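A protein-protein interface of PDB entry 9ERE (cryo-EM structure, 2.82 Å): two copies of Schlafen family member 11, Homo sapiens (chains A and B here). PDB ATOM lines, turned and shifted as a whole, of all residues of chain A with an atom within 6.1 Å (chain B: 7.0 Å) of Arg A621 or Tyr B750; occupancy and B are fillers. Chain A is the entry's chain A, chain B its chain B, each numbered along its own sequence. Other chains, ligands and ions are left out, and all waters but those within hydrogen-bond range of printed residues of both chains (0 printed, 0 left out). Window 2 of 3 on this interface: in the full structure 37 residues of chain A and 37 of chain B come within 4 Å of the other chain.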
ATOM      1  N   SER A 616       5.649  34.766 -35.717  1.00  0.00           N
ATOM      2  CA  SER A 616       4.464  34.234 -35.061  1.00  0.00           C
ATOM      3  C   SER A 616       4.646  32.798 -34.597  1.00  0.00           C
ATOM      4  O   SER A 616       3.811  32.305 -33.833  1.00  0.00           O
ATOM      5  CB  SER A 616       3.267  34.312 -36.008  1.00  0.00           C
ATOM      6  OG  SER A 616       2.947  35.655 -36.318  1.00  0.00           O
ATOM      7  N   LEU A 617       5.699  32.112 -35.043  1.00  0.00           N
ATOM      8  CA  LEU A 617       5.906  30.730 -34.621  1.00  0.00           C
ATOM      9  C   LEU A 617       6.208  30.650 -33.132  1.00  0.00           C
ATOM     10  O   LEU A 617       5.709  29.759 -32.437  1.00  0.00           O
ATOM     11  CB  LEU A 617       7.036  30.099 -35.432  1.00  0.00           C
ATOM     12  CG  LEU A 617       7.231  28.599 -35.217  1.00  0.00           C
ATOM     13  CD1 LEU A 617       6.038  27.828 -35.747  1.00  0.00           C
ATOM     14  CD2 LEU A 617       8.510  28.126 -35.877  1.00  0.00           C
ATOM     15  N   ARG A 618       7.028  31.571 -32.628  1.00  0.00           N
ATOM     16  CA  ARG A 618       7.348  31.617 -31.209  1.00  0.00           C
ATOM     17  C   ARG A 618       6.158  32.035 -30.358  1.00  0.00           C
ATOM     18  O   ARG A 618       6.211  31.885 -29.133  1.00  0.00           O
ATOM     19  CB  ARG A 618       8.525  32.575 -30.995  1.00  0.00           C
ATOM     20  CG  ARG A 618       8.610  33.215 -29.620  1.00  0.00           C
ATOM     21  CD  ARG A 618       9.888  34.040 -29.481  1.00  0.00           C
ATOM     22  NE  ARG A 618      10.264  34.305 -28.096  1.00  0.00           N
ATOM     23  CZ  ARG A 618      10.479  33.380 -27.169  1.00  0.00           C
ATOM     24  NH1 ARG A 618      10.461  32.088 -27.458  1.00  0.00           N
ATOM     25  NH2 ARG A 618      10.740  33.762 -25.922  1.00  0.00           N
ATOM     26  N   LYS A 619       5.082  32.524 -30.973  1.00  0.00           N
ATOM     27  CA  LYS A 619       3.970  33.108 -30.242  1.00  0.00           C
ATOM     28  C   LYS A 619       2.670  32.329 -30.358  1.00  0.00           C
ATOM     29  O   LYS A 619       1.780  32.533 -29.528  1.00  0.00           O
ATOM     30  CB  LYS A 619       3.729  34.542 -30.731  1.00  0.00           C
ATOM     31  CG  LYS A 619       4.969  35.409 -30.655  1.00  0.00           C
ATOM     32  CD  LYS A 619       4.652  36.878 -30.811  1.00  0.00           C
ATOM     33  CE  LYS A 619       4.118  37.189 -32.192  1.00  0.00           C
ATOM     34  NZ  LYS A 619       4.124  38.649 -32.465  1.00  0.00           N
ATOM     35  N   ASN A 620       2.537  31.447 -31.345  1.00  0.00           N
ATOM     36  CA  ASN A 620       1.299  30.719 -31.583  1.00  0.00           C
ATOM     37  C   ASN A 620       1.580  29.230 -31.706  1.00  0.00           C
ATOM     38  O   ASN A 620       2.554  28.825 -32.344  1.00  0.00           O
ATOM     39  CB  ASN A 620       0.604  31.208 -32.855  1.00  0.00           C
ATOM     40  CG  ASN A 620       0.266  32.682 -32.807  1.00  0.00           C
ATOM     41  OD1 ASN A 620      -0.761  33.076 -32.263  1.00  0.00           O
ATOM     42  ND2 ASN A 620       1.128  33.504 -33.384  1.00  0.00           N
ATOM     43  N   ARG A 621       0.728  28.422 -31.079  1.00  0.00           N
ATOM     44  CA  ARG A 621       0.732  26.983 -31.308  1.00  0.00           C
ATOM     45  C   ARG A 621      -0.319  26.653 -32.357  1.00  0.00           C
ATOM     46  O   ARG A 621      -0.003  26.084 -33.404  1.00  0.00           O
ATOM     47  CB  ARG A 621       0.457  26.215 -30.010  1.00  0.00           C
ATOM     48  CG  ARG A 621       1.667  25.548 -29.341  1.00  0.00           C
ATOM     49  CD  ARG A 621       2.989  26.249 -29.615  1.00  0.00           C
ATOM     50  NE  ARG A 621       4.111  25.575 -28.977  1.00  0.00           N
ATOM     51  CZ  ARG A 621       5.367  25.993 -29.050  1.00  0.00           C
ATOM     52  NH1 ARG A 621       5.693  27.086 -29.723  1.00  0.00           N
ATOM     53  NH2 ARG A 621       6.319  25.299 -28.436  1.00  0.00           N
ATOM     54  N   GLU A 622      -1.568  27.011 -32.081  1.00  0.00           N
ATOM     55  CA  GLU A 622      -2.616  26.953 -33.086  1.00  0.00           C
ATOM     56  C   GLU A 622      -2.773  28.322 -33.728  1.00  0.00           C
ATOM     57  O   GLU A 622      -2.901  29.334 -33.038  1.00  0.00           O
ATOM     58  CB  GLU A 622      -3.941  26.519 -32.460  1.00  0.00           C
ATOM     59  CG  GLU A 622      -3.887  25.177 -31.756  1.00  0.00           C
ATOM     60  CD  GLU A 622      -5.265  24.645 -31.416  1.00  0.00           C
ATOM     61  OE1 GLU A 622      -6.262  25.327 -31.734  1.00  0.00           O
ATOM     62  OE2 GLU A 622      -5.352  23.547 -30.826  1.00  0.00           O
ATOM     63  N   LEU A 623      -2.757  28.352 -35.056  1.00  0.00           N
ATOM     64  CA  LEU A 623      -2.859  29.605 -35.786  1.00  0.00           C
ATOM     65  C   LEU A 623      -3.578  29.356 -37.100  1.00  0.00           C
ATOM     66  O   LEU A 623      -3.271  28.397 -37.811  1.00  0.00           O
ATOM     67  CB  LEU A 623      -1.474  30.210 -36.044  1.00  0.00           C
ATOM     68  CG  LEU A 623      -1.433  31.560 -36.759  1.00  0.00           C
ATOM     69  CD1 LEU A 623      -2.083  32.633 -35.922  1.00  0.00           C
ATOM     70  CD2 LEU A 623      -0.008  31.938 -37.084  1.00  0.00           C
ATOM     71  N   PHE A 648      12.109  23.466 -33.115  1.00  0.00           N
ATOM     72  CA  PHE A 648      11.709  22.398 -32.208  1.00  0.00           C
ATOM     73  C   PHE A 648      12.628  21.188 -32.306  1.00  0.00           C
ATOM     74  O   PHE A 648      12.429  20.211 -31.577  1.00  0.00           O
ATOM     75  CB  PHE A 648      10.265  21.956 -32.457  1.00  0.00           C
ATOM     76  CG  PHE A 648       9.223  23.000 -32.135  1.00  0.00           C
ATOM     77  CD1 PHE A 648       9.346  24.308 -32.576  1.00  0.00           C
ATOM     78  CD2 PHE A 648       8.075  22.644 -31.448  1.00  0.00           C
ATOM     79  CE1 PHE A 648       8.367  25.244 -32.295  1.00  0.00           C
ATOM     80  CE2 PHE A 648       7.101  23.576 -31.160  1.00  0.00           C
ATOM     81  CZ  PHE A 648       7.244  24.874 -31.587  1.00  0.00           C
ATOM     82  N   PRO A 723       2.235  20.265 -26.265  1.00  0.00           N
ATOM     83  CA  PRO A 723       1.384  20.493 -27.439  1.00  0.00           C
ATOM     84  C   PRO A 723       2.198  21.049 -28.598  1.00  0.00           C
ATOM     85  O   PRO A 723       3.104  21.863 -28.411  1.00  0.00           O
ATOM     86  CB  PRO A 723       0.338  21.497 -26.936  1.00  0.00           C
ATOM     87  CG  PRO A 723       0.911  22.075 -25.685  1.00  0.00           C
ATOM     88  CD  PRO A 723       1.757  21.003 -25.086  1.00  0.00           C
ATOM     89  N   GLY A 724       1.872  20.588 -29.807  1.00  0.00           N
ATOM     90  CA  GLY A 724       2.622  20.949 -30.988  1.00  0.00           C
ATOM     91  C   GLY A 724       1.966  22.055 -31.790  1.00  0.00           C
ATOM     92  O   GLY A 724       0.942  22.624 -31.414  1.00  0.00           O
ATOM     93  N   ILE A 725       2.590  22.357 -32.928  1.00  0.00           N
ATOM     94  CA  ILE A 725       2.083  23.383 -33.827  1.00  0.00           C
ATOM     95  C   ILE A 725       0.922  22.826 -34.635  1.00  0.00           C
ATOM     96  O   ILE A 725       0.984  21.708 -35.161  1.00  0.00           O
ATOM     97  CB  ILE A 725       3.209  23.874 -34.753  1.00  0.00           C
ATOM     98  CG1 ILE A 725       4.388  24.418 -33.944  1.00  0.00           C
ATOM     99  CG2 ILE A 725       2.700  24.944 -35.687  1.00  0.00           C
ATOM    100  CD1 ILE A 725       4.060  25.627 -33.114  1.00  0.00           C
ATOM    101  N   LEU A 726      -0.154  23.605 -34.734  1.00  0.00           N
ATOM    102  CA  LEU A 726      -1.276  23.301 -35.621  1.00  0.00           C
ATOM    103  C   LEU A 726      -1.602  24.580 -36.377  1.00  0.00           C
ATOM    104  O   LEU A 726      -2.473  25.347 -35.963  1.00  0.00           O
ATOM    105  CB  LEU A 726      -2.484  22.792 -34.851  1.00  0.00           C
ATOM    106  CG  LEU A 726      -3.725  22.553 -35.714  1.00  0.00           C
ATOM    107  CD1 LEU A 726      -3.450  21.487 -36.755  1.00  0.00           C
ATOM    108  CD2 LEU A 726      -4.910  22.169 -34.856  1.00  0.00           C
ATOM    109  N   TRP A 727      -0.925  24.797 -37.499  1.00  0.00           N
ATOM    110  CA  TRP A 727      -1.150  25.970 -38.326  1.00  0.00           C
ATOM    111  C   TRP A 727      -1.982  25.575 -39.535  1.00  0.00           C
ATOM    112  O   TRP A 727      -1.626  24.647 -40.265  1.00  0.00           O
ATOM    113  CB  TRP A 727       0.176  26.598 -38.756  1.00  0.00           C
ATOM    114  CG  TRP A 727       0.785  27.418 -37.665  1.00  0.00           C
ATOM    115  CD1 TRP A 727       0.564  27.283 -36.329  1.00  0.00           C
ATOM    116  CD2 TRP A 727       1.698  28.509 -37.810  1.00  0.00           C
ATOM    117  NE1 TRP A 727       1.287  28.212 -35.631  1.00  0.00           N
ATOM    118  CE2 TRP A 727       1.990  28.981 -36.519  1.00  0.00           C
ATOM    119  CE3 TRP A 727       2.295  29.134 -38.904  1.00  0.00           C
ATOM    120  CZ2 TRP A 727       2.854  30.044 -36.292  1.00  0.00           C
ATOM    121  CZ3 TRP A 727       3.151  30.193 -38.675  1.00  0.00           C
ATOM    122  CH2 TRP A 727       3.424  30.635 -37.382  1.00  0.00           C
ATOM    123  N   PRO A 751      -6.030  32.000 -32.771  1.00  0.00           N
ATOM    124  CA  PRO A 751      -5.497  33.294 -33.219  1.00  0.00           C
ATOM    125  C   PRO A 751      -5.360  33.341 -34.733  1.00  0.00           C
ATOM    126  O   PRO A 751      -5.400  32.308 -35.389  1.00  0.00           O
ATOM    127  CB  PRO A 751      -4.141  33.374 -32.508  1.00  0.00           C
ATOM    128  CG  PRO A 751      -3.734  31.964 -32.314  1.00  0.00           C
ATOM    129  CD  PRO A 751      -5.014  31.226 -32.039  1.00  0.00           C
ATOM    130  N   ASN B 620      -5.792  38.150 -32.013  1.00  0.00           N
ATOM    131  CA  ASN B 620      -5.983  37.264 -30.876  1.00  0.00           C
ATOM    132  C   ASN B 620      -7.282  37.604 -30.166  1.00  0.00           C
ATOM    133  O   ASN B 620      -7.744  38.746 -30.176  1.00  0.00           O
ATOM    134  CB  ASN B 620      -4.820  37.366 -29.885  1.00  0.00           C
ATOM    135  CG  ASN B 620      -3.495  36.997 -30.503  1.00  0.00           C
ATOM    136  OD1 ASN B 620      -3.145  35.825 -30.595  1.00  0.00           O
ATOM    137  ND2 ASN B 620      -2.746  38.002 -30.931  1.00  0.00           N
ATOM    138  N   GLU B 622      -7.923  35.158 -27.038  1.00  0.00           N
ATOM    139  CA  GLU B 622      -7.094  34.840 -25.888  1.00  0.00           C
ATOM    140  C   GLU B 622      -5.651  35.204 -26.192  1.00  0.00           C
ATOM    141  O   GLU B 622      -5.145  34.937 -27.284  1.00  0.00           O
ATOM    142  CB  GLU B 622      -7.197  33.356 -25.547  1.00  0.00           C
ATOM    143  CG  GLU B 622      -8.319  33.025 -24.591  1.00  0.00           C
ATOM    144  CD  GLU B 622      -9.656  32.887 -25.286  1.00  0.00           C
ATOM    145  OE1 GLU B 622     -10.430  33.866 -25.289  1.00  0.00           O
ATOM    146  OE2 GLU B 622      -9.936  31.797 -25.826  1.00  0.00           O
ATOM    147  N   LEU B 623      -4.988  35.826 -25.224  1.00  0.00           N
ATOM    148  CA  LEU B 623      -3.585  36.196 -25.387  1.00  0.00           C
ATOM    149  C   LEU B 623      -2.973  36.330 -24.007  1.00  0.00           C
ATOM    150  O   LEU B 623      -3.459  37.119 -23.191  1.00  0.00           O
ATOM    151  CB  LEU B 623      -3.448  37.499 -26.173  1.00  0.00           C
ATOM    152  CG  LEU B 623      -2.023  37.978 -26.453  1.00  0.00           C
ATOM    153  CD1 LEU B 623      -1.294  37.004 -27.341  1.00  0.00           C
ATOM    154  CD2 LEU B 623      -2.045  39.348 -27.087  1.00  0.00           C
ATOM    155  N   PHE B 624      -1.921  35.563 -23.744  1.00  0.00           N
ATOM    156  CA  PHE B 624      -1.170  35.664 -22.500  1.00  0.00           C
ATOM    157  C   PHE B 624       0.045  36.546 -22.747  1.00  0.00           C
ATOM    158  O   PHE B 624       0.961  36.162 -23.478  1.00  0.00           O
ATOM    159  CB  PHE B 624      -0.758  34.284 -22.003  1.00  0.00           C
ATOM    160  CG  PHE B 624      -1.909  33.431 -21.572  1.00  0.00           C
ATOM    161  CD1 PHE B 624      -2.676  32.758 -22.503  1.00  0.00           C
ATOM    162  CD2 PHE B 624      -2.226  33.302 -20.237  1.00  0.00           C
ATOM    163  CE1 PHE B 624      -3.735  31.975 -22.107  1.00  0.00           C
ATOM    164  CE2 PHE B 624      -3.281  32.519 -19.838  1.00  0.00           C
ATOM    165  CZ  PHE B 624      -4.038  31.857 -20.775  1.00  0.00           C
ATOM    166  N   TYR B 709      -9.624  31.846 -13.679  1.00  0.00           N
ATOM    167  CA  TYR B 709      -9.407  31.632 -15.103  1.00  0.00           C
ATOM    168  C   TYR B 709     -10.644  31.037 -15.756  1.00  0.00           C
ATOM    169  O   TYR B 709     -11.060  31.482 -16.831  1.00  0.00           O
ATOM    170  CB  TYR B 709      -8.224  30.697 -15.340  1.00  0.00           C
ATOM    171  CG  TYR B 709      -7.821  30.578 -16.798  1.00  0.00           C
ATOM    172  CD1 TYR B 709      -8.352  31.425 -17.765  1.00  0.00           C
ATOM    173  CD2 TYR B 709      -6.970  29.571 -17.221  1.00  0.00           C
ATOM    174  CE1 TYR B 709      -7.996  31.312 -19.090  1.00  0.00           C
ATOM    175  CE2 TYR B 709      -6.619  29.445 -18.550  1.00  0.00           C
ATOM    176  CZ  TYR B 709      -7.137  30.318 -19.479  1.00  0.00           C
ATOM    177  OH  TYR B 709      -6.793  30.201 -20.805  1.00  0.00           O
ATOM    178  N   PRO B 744      -3.170  28.701 -16.361  1.00  0.00           N
ATOM    179  CA  PRO B 744      -2.995  27.436 -17.058  1.00  0.00           C
ATOM    180  C   PRO B 744      -1.523  27.081 -17.144  1.00  0.00           C
ATOM    181  O   PRO B 744      -0.661  27.961 -17.009  1.00  0.00           O
ATOM    182  CB  PRO B 744      -3.587  27.713 -18.444  1.00  0.00           C
ATOM    183  CG  PRO B 744      -3.377  29.156 -18.640  1.00  0.00           C
ATOM    184  CD  PRO B 744      -3.514  29.793 -17.288  1.00  0.00           C
ATOM    185  N   PRO B 745      -1.190  25.810 -17.353  1.00  0.00           N
ATOM    186  CA  PRO B 745       0.220  25.443 -17.506  1.00  0.00           C
ATOM    187  C   PRO B 745       0.903  26.325 -18.542  1.00  0.00           C
ATOM    188  O   PRO B 745       0.252  26.950 -19.384  1.00  0.00           O
ATOM    189  CB  PRO B 745       0.160  23.980 -17.954  1.00  0.00           C
ATOM    190  CG  PRO B 745      -1.136  23.479 -17.426  1.00  0.00           C
ATOM    191  CD  PRO B 745      -2.081  24.643 -17.461  1.00  0.00           C
ATOM    192  N   LEU B 746       2.233  26.385 -18.466  1.00  0.00           N
ATOM    193  CA  LEU B 746       2.972  27.231 -19.396  1.00  0.00           C
ATOM    194  C   LEU B 746       2.761  26.789 -20.836  1.00  0.00           C
ATOM    195  O   LEU B 746       2.605  27.632 -21.726  1.00  0.00           O
ATOM    196  CB  LEU B 746       4.460  27.221 -19.052  1.00  0.00           C
ATOM    197  CG  LEU B 746       5.326  28.354 -19.615  1.00  0.00           C
ATOM    198  CD1 LEU B 746       4.592  29.686 -19.665  1.00  0.00           C
ATOM    199  CD2 LEU B 746       6.592  28.485 -18.800  1.00  0.00           C
ATOM    200  N   SER B 747       2.756  25.480 -21.086  1.00  0.00           N
ATOM    201  CA  SER B 747       2.469  24.986 -22.426  1.00  0.00           C
ATOM    202  C   SER B 747       1.084  25.400 -22.899  1.00  0.00           C
ATOM    203  O   SER B 747       0.884  25.595 -24.103  1.00  0.00           O
ATOM    204  CB  SER B 747       2.589  23.465 -22.456  1.00  0.00           C
ATOM    205  OG  SER B 747       1.778  22.875 -21.456  1.00  0.00           O
ATOM    206  N   ASP B 748       0.131  25.537 -21.981  1.00  0.00           N
ATOM    207  CA  ASP B 748      -1.226  25.950 -22.298  1.00  0.00           C
ATOM    208  C   ASP B 748      -1.339  27.457 -22.505  1.00  0.00           C
ATOM    209  O   ASP B 748      -2.226  27.903 -23.237  1.00  0.00           O
ATOM    210  CB  ASP B 748      -2.164  25.486 -21.171  1.00  0.00           C
ATOM    211  CG  ASP B 748      -3.632  25.816 -21.419  1.00  0.00           C
ATOM    212  OD1 ASP B 748      -3.951  26.791 -22.126  1.00  0.00           O
ATOM    213  OD2 ASP B 748      -4.484  25.084 -20.876  1.00  0.00           O
ATOM    214  N   GLN B 749      -0.435  28.241 -21.921  1.00  0.00           N
ATOM    215  CA  GLN B 749      -0.487  29.701 -22.025  1.00  0.00           C
ATOM    216  C   GLN B 749      -0.102  30.129 -23.439  1.00  0.00           C
ATOM    217  O   GLN B 749       1.009  30.590 -23.703  1.00  0.00           O
ATOM    218  CB  GLN B 749       0.437  30.342 -20.997  1.00  0.00           C
ATOM    219  CG  GLN B 749      -0.076  30.296 -19.575  1.00  0.00           C
ATOM    220  CD  GLN B 749       0.919  30.860 -18.589  1.00  0.00           C
ATOM    221  OE1 GLN B 749       1.654  31.792 -18.903  1.00  0.00           O
ATOM    222  NE2 GLN B 749       0.948  30.299 -17.388  1.00  0.00           N
ATOM    223  N   TYR B 750      -1.046  29.975 -24.364  1.00  0.00           N
ATOM    224  CA  TYR B 750      -0.886  30.426 -25.740  1.00  0.00           C
ATOM    225  C   TYR B 750      -2.216  30.947 -26.261  1.00  0.00           C
ATOM    226  O   TYR B 750      -3.276  30.524 -25.790  1.00  0.00           O
ATOM    227  CB  TYR B 750      -0.384  29.302 -26.656  1.00  0.00           C
ATOM    228  CG  TYR B 750       1.105  29.090 -26.585  1.00  0.00           C
ATOM    229  CD1 TYR B 750       1.977  29.959 -27.217  1.00  0.00           C
ATOM    230  CD2 TYR B 750       1.638  28.024 -25.886  1.00  0.00           C
ATOM    231  CE1 TYR B 750       3.337  29.774 -27.150  1.00  0.00           C
ATOM    232  CE2 TYR B 750       2.996  27.830 -25.812  1.00  0.00           C
ATOM    233  CZ  TYR B 750       3.842  28.708 -26.448  1.00  0.00           C
ATOM    234  OH  TYR B 750       5.201  28.517 -26.380  1.00  0.00           O
ATOM    235  N   PRO B 751      -2.192  31.871 -27.230  1.00  0.00           N
ATOM    236  CA  PRO B 751      -1.020  32.512 -27.845  1.00  0.00           C
ATOM    237  C   PRO B 751      -0.345  33.493 -26.895  1.00  0.00           C
ATOM    238  O   PRO B 751      -0.970  33.996 -25.970  1.00  0.00           O
ATOM    239  CB  PRO B 751      -1.618  33.215 -29.067  1.00  0.00           C
ATOM    240  CG  PRO B 751      -3.018  33.520 -28.669  1.00  0.00           C
ATOM    241  CD  PRO B 751      -3.447  32.353 -27.829  1.00  0.00           C
ATOM    242  N   ARG B 752       0.935  33.782 -27.103  1.00  0.00           N
ATOM    243  CA  ARG B 752       1.704  34.625 -26.206  1.00  0.00           C
ATOM    244  C   ARG B 752       2.193  35.870 -26.927  1.00  0.00           C
ATOM    245  O   ARG B 752       2.485  35.852 -28.124  1.00  0.00           O
ATOM    246  CB  ARG B 752       2.916  33.885 -25.642  1.00  0.00           C
ATOM    247  CG  ARG B 752       2.587  32.850 -24.606  1.00  0.00           C
ATOM    248  CD  ARG B 752       3.823  32.476 -23.827  1.00  0.00           C
ATOM    249  NE  ARG B 752       3.781  31.089 -23.386  1.00  0.00           N
ATOM    250  CZ  ARG B 752       4.850  30.330 -23.195  1.00  0.00           C
ATOM    251  NH1 ARG B 752       6.074  30.797 -23.382  1.00  0.00           N
ATOM    252  NH2 ARG B 752       4.691  29.067 -22.810  1.00  0.00           N
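O of Lys A619 lies within hydrogen-bond range of N of Arg B752 (2.9 Å).
NH2 of Arg B752 sits at hydrogen-bond distance from O of Leu B746 (2.8 Å). The backbone carbonyl oxygen (O) of Arg A621 sits close to the indole nitrogen (NE1) of Trp A727 (3.3 Å). The guanidinium group of Arg B752 is in hydrogen-bond range of the backbone carbonyl oxygen of Gln B749 (2.8 Å). The backbone carbonyl oxygen of Arg A621 sits at hydrogen-bond distance from the backbone NH of Leu A726 (2.8 Å). The backbone carbonyl oxygen of Ser A616 is in hydrogen-bond range of the side-chain amide nitrogen of Asn A620 (3.0 Å). The backbone NH of Phe B624 lies within hydrogen-bond range of the backbone carbonyl oxygen of Pro B751, 2.9 Å away.
Tyr B750 touches Lys A619 (CD1 to O, 3.5 Å). Lys A619 touches Pro B751. Pro B751 touches Asn A620. Arg A621 touches Tyr B750. Ser B747 touches Pro A723. Asn B620 touches Pro A751.
Arg A621 touches one residue of chain B. Of the printed residues of chain B, Asn A620 touches Pro B751 (3.3 Å). Printed residues of chain A within 4 Å of Ser B747: Pro A723 (3.7 Å). Of the printed residues of chain B, Pro A723 touches Ser B747 (3.7 Å). Printed residues of chain B within 4 Å of Lys A619: Tyr B750 (3.5 Å), Pro B751 (3.3 Å) and Arg B752 (2.9 Å). The nearest residue of chain B that does not touch Arg A621 is Ser B747 (5.3 Å). The nearest residue of chain A that does not touch Tyr B750 is Arg A618 (4.1 Å). The nearest printed residue of chain A that does not touch Asn B620 is Asn A620 (4.003 Å).
Printed residues of chain A that touch a printed residue of chain B: Lys A619, Asn A620, Arg A621, Pro A723 and Pro A751. Among the printed residues, 7 pairs touch across the chains. Among the printed residues, no Asp or Glu carboxylate lies within 4 Å of a Lys or Arg side-chain nitrogen of the other chain.
Asn A620 touches Pro B751, and with the chains exchanged Pro A751 touches Asn B620. 4 positions are printed for both chains. Of the 7 pairs that touch across the chains among the printed residues, 2 have their exchanged pair printed and touching as well.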
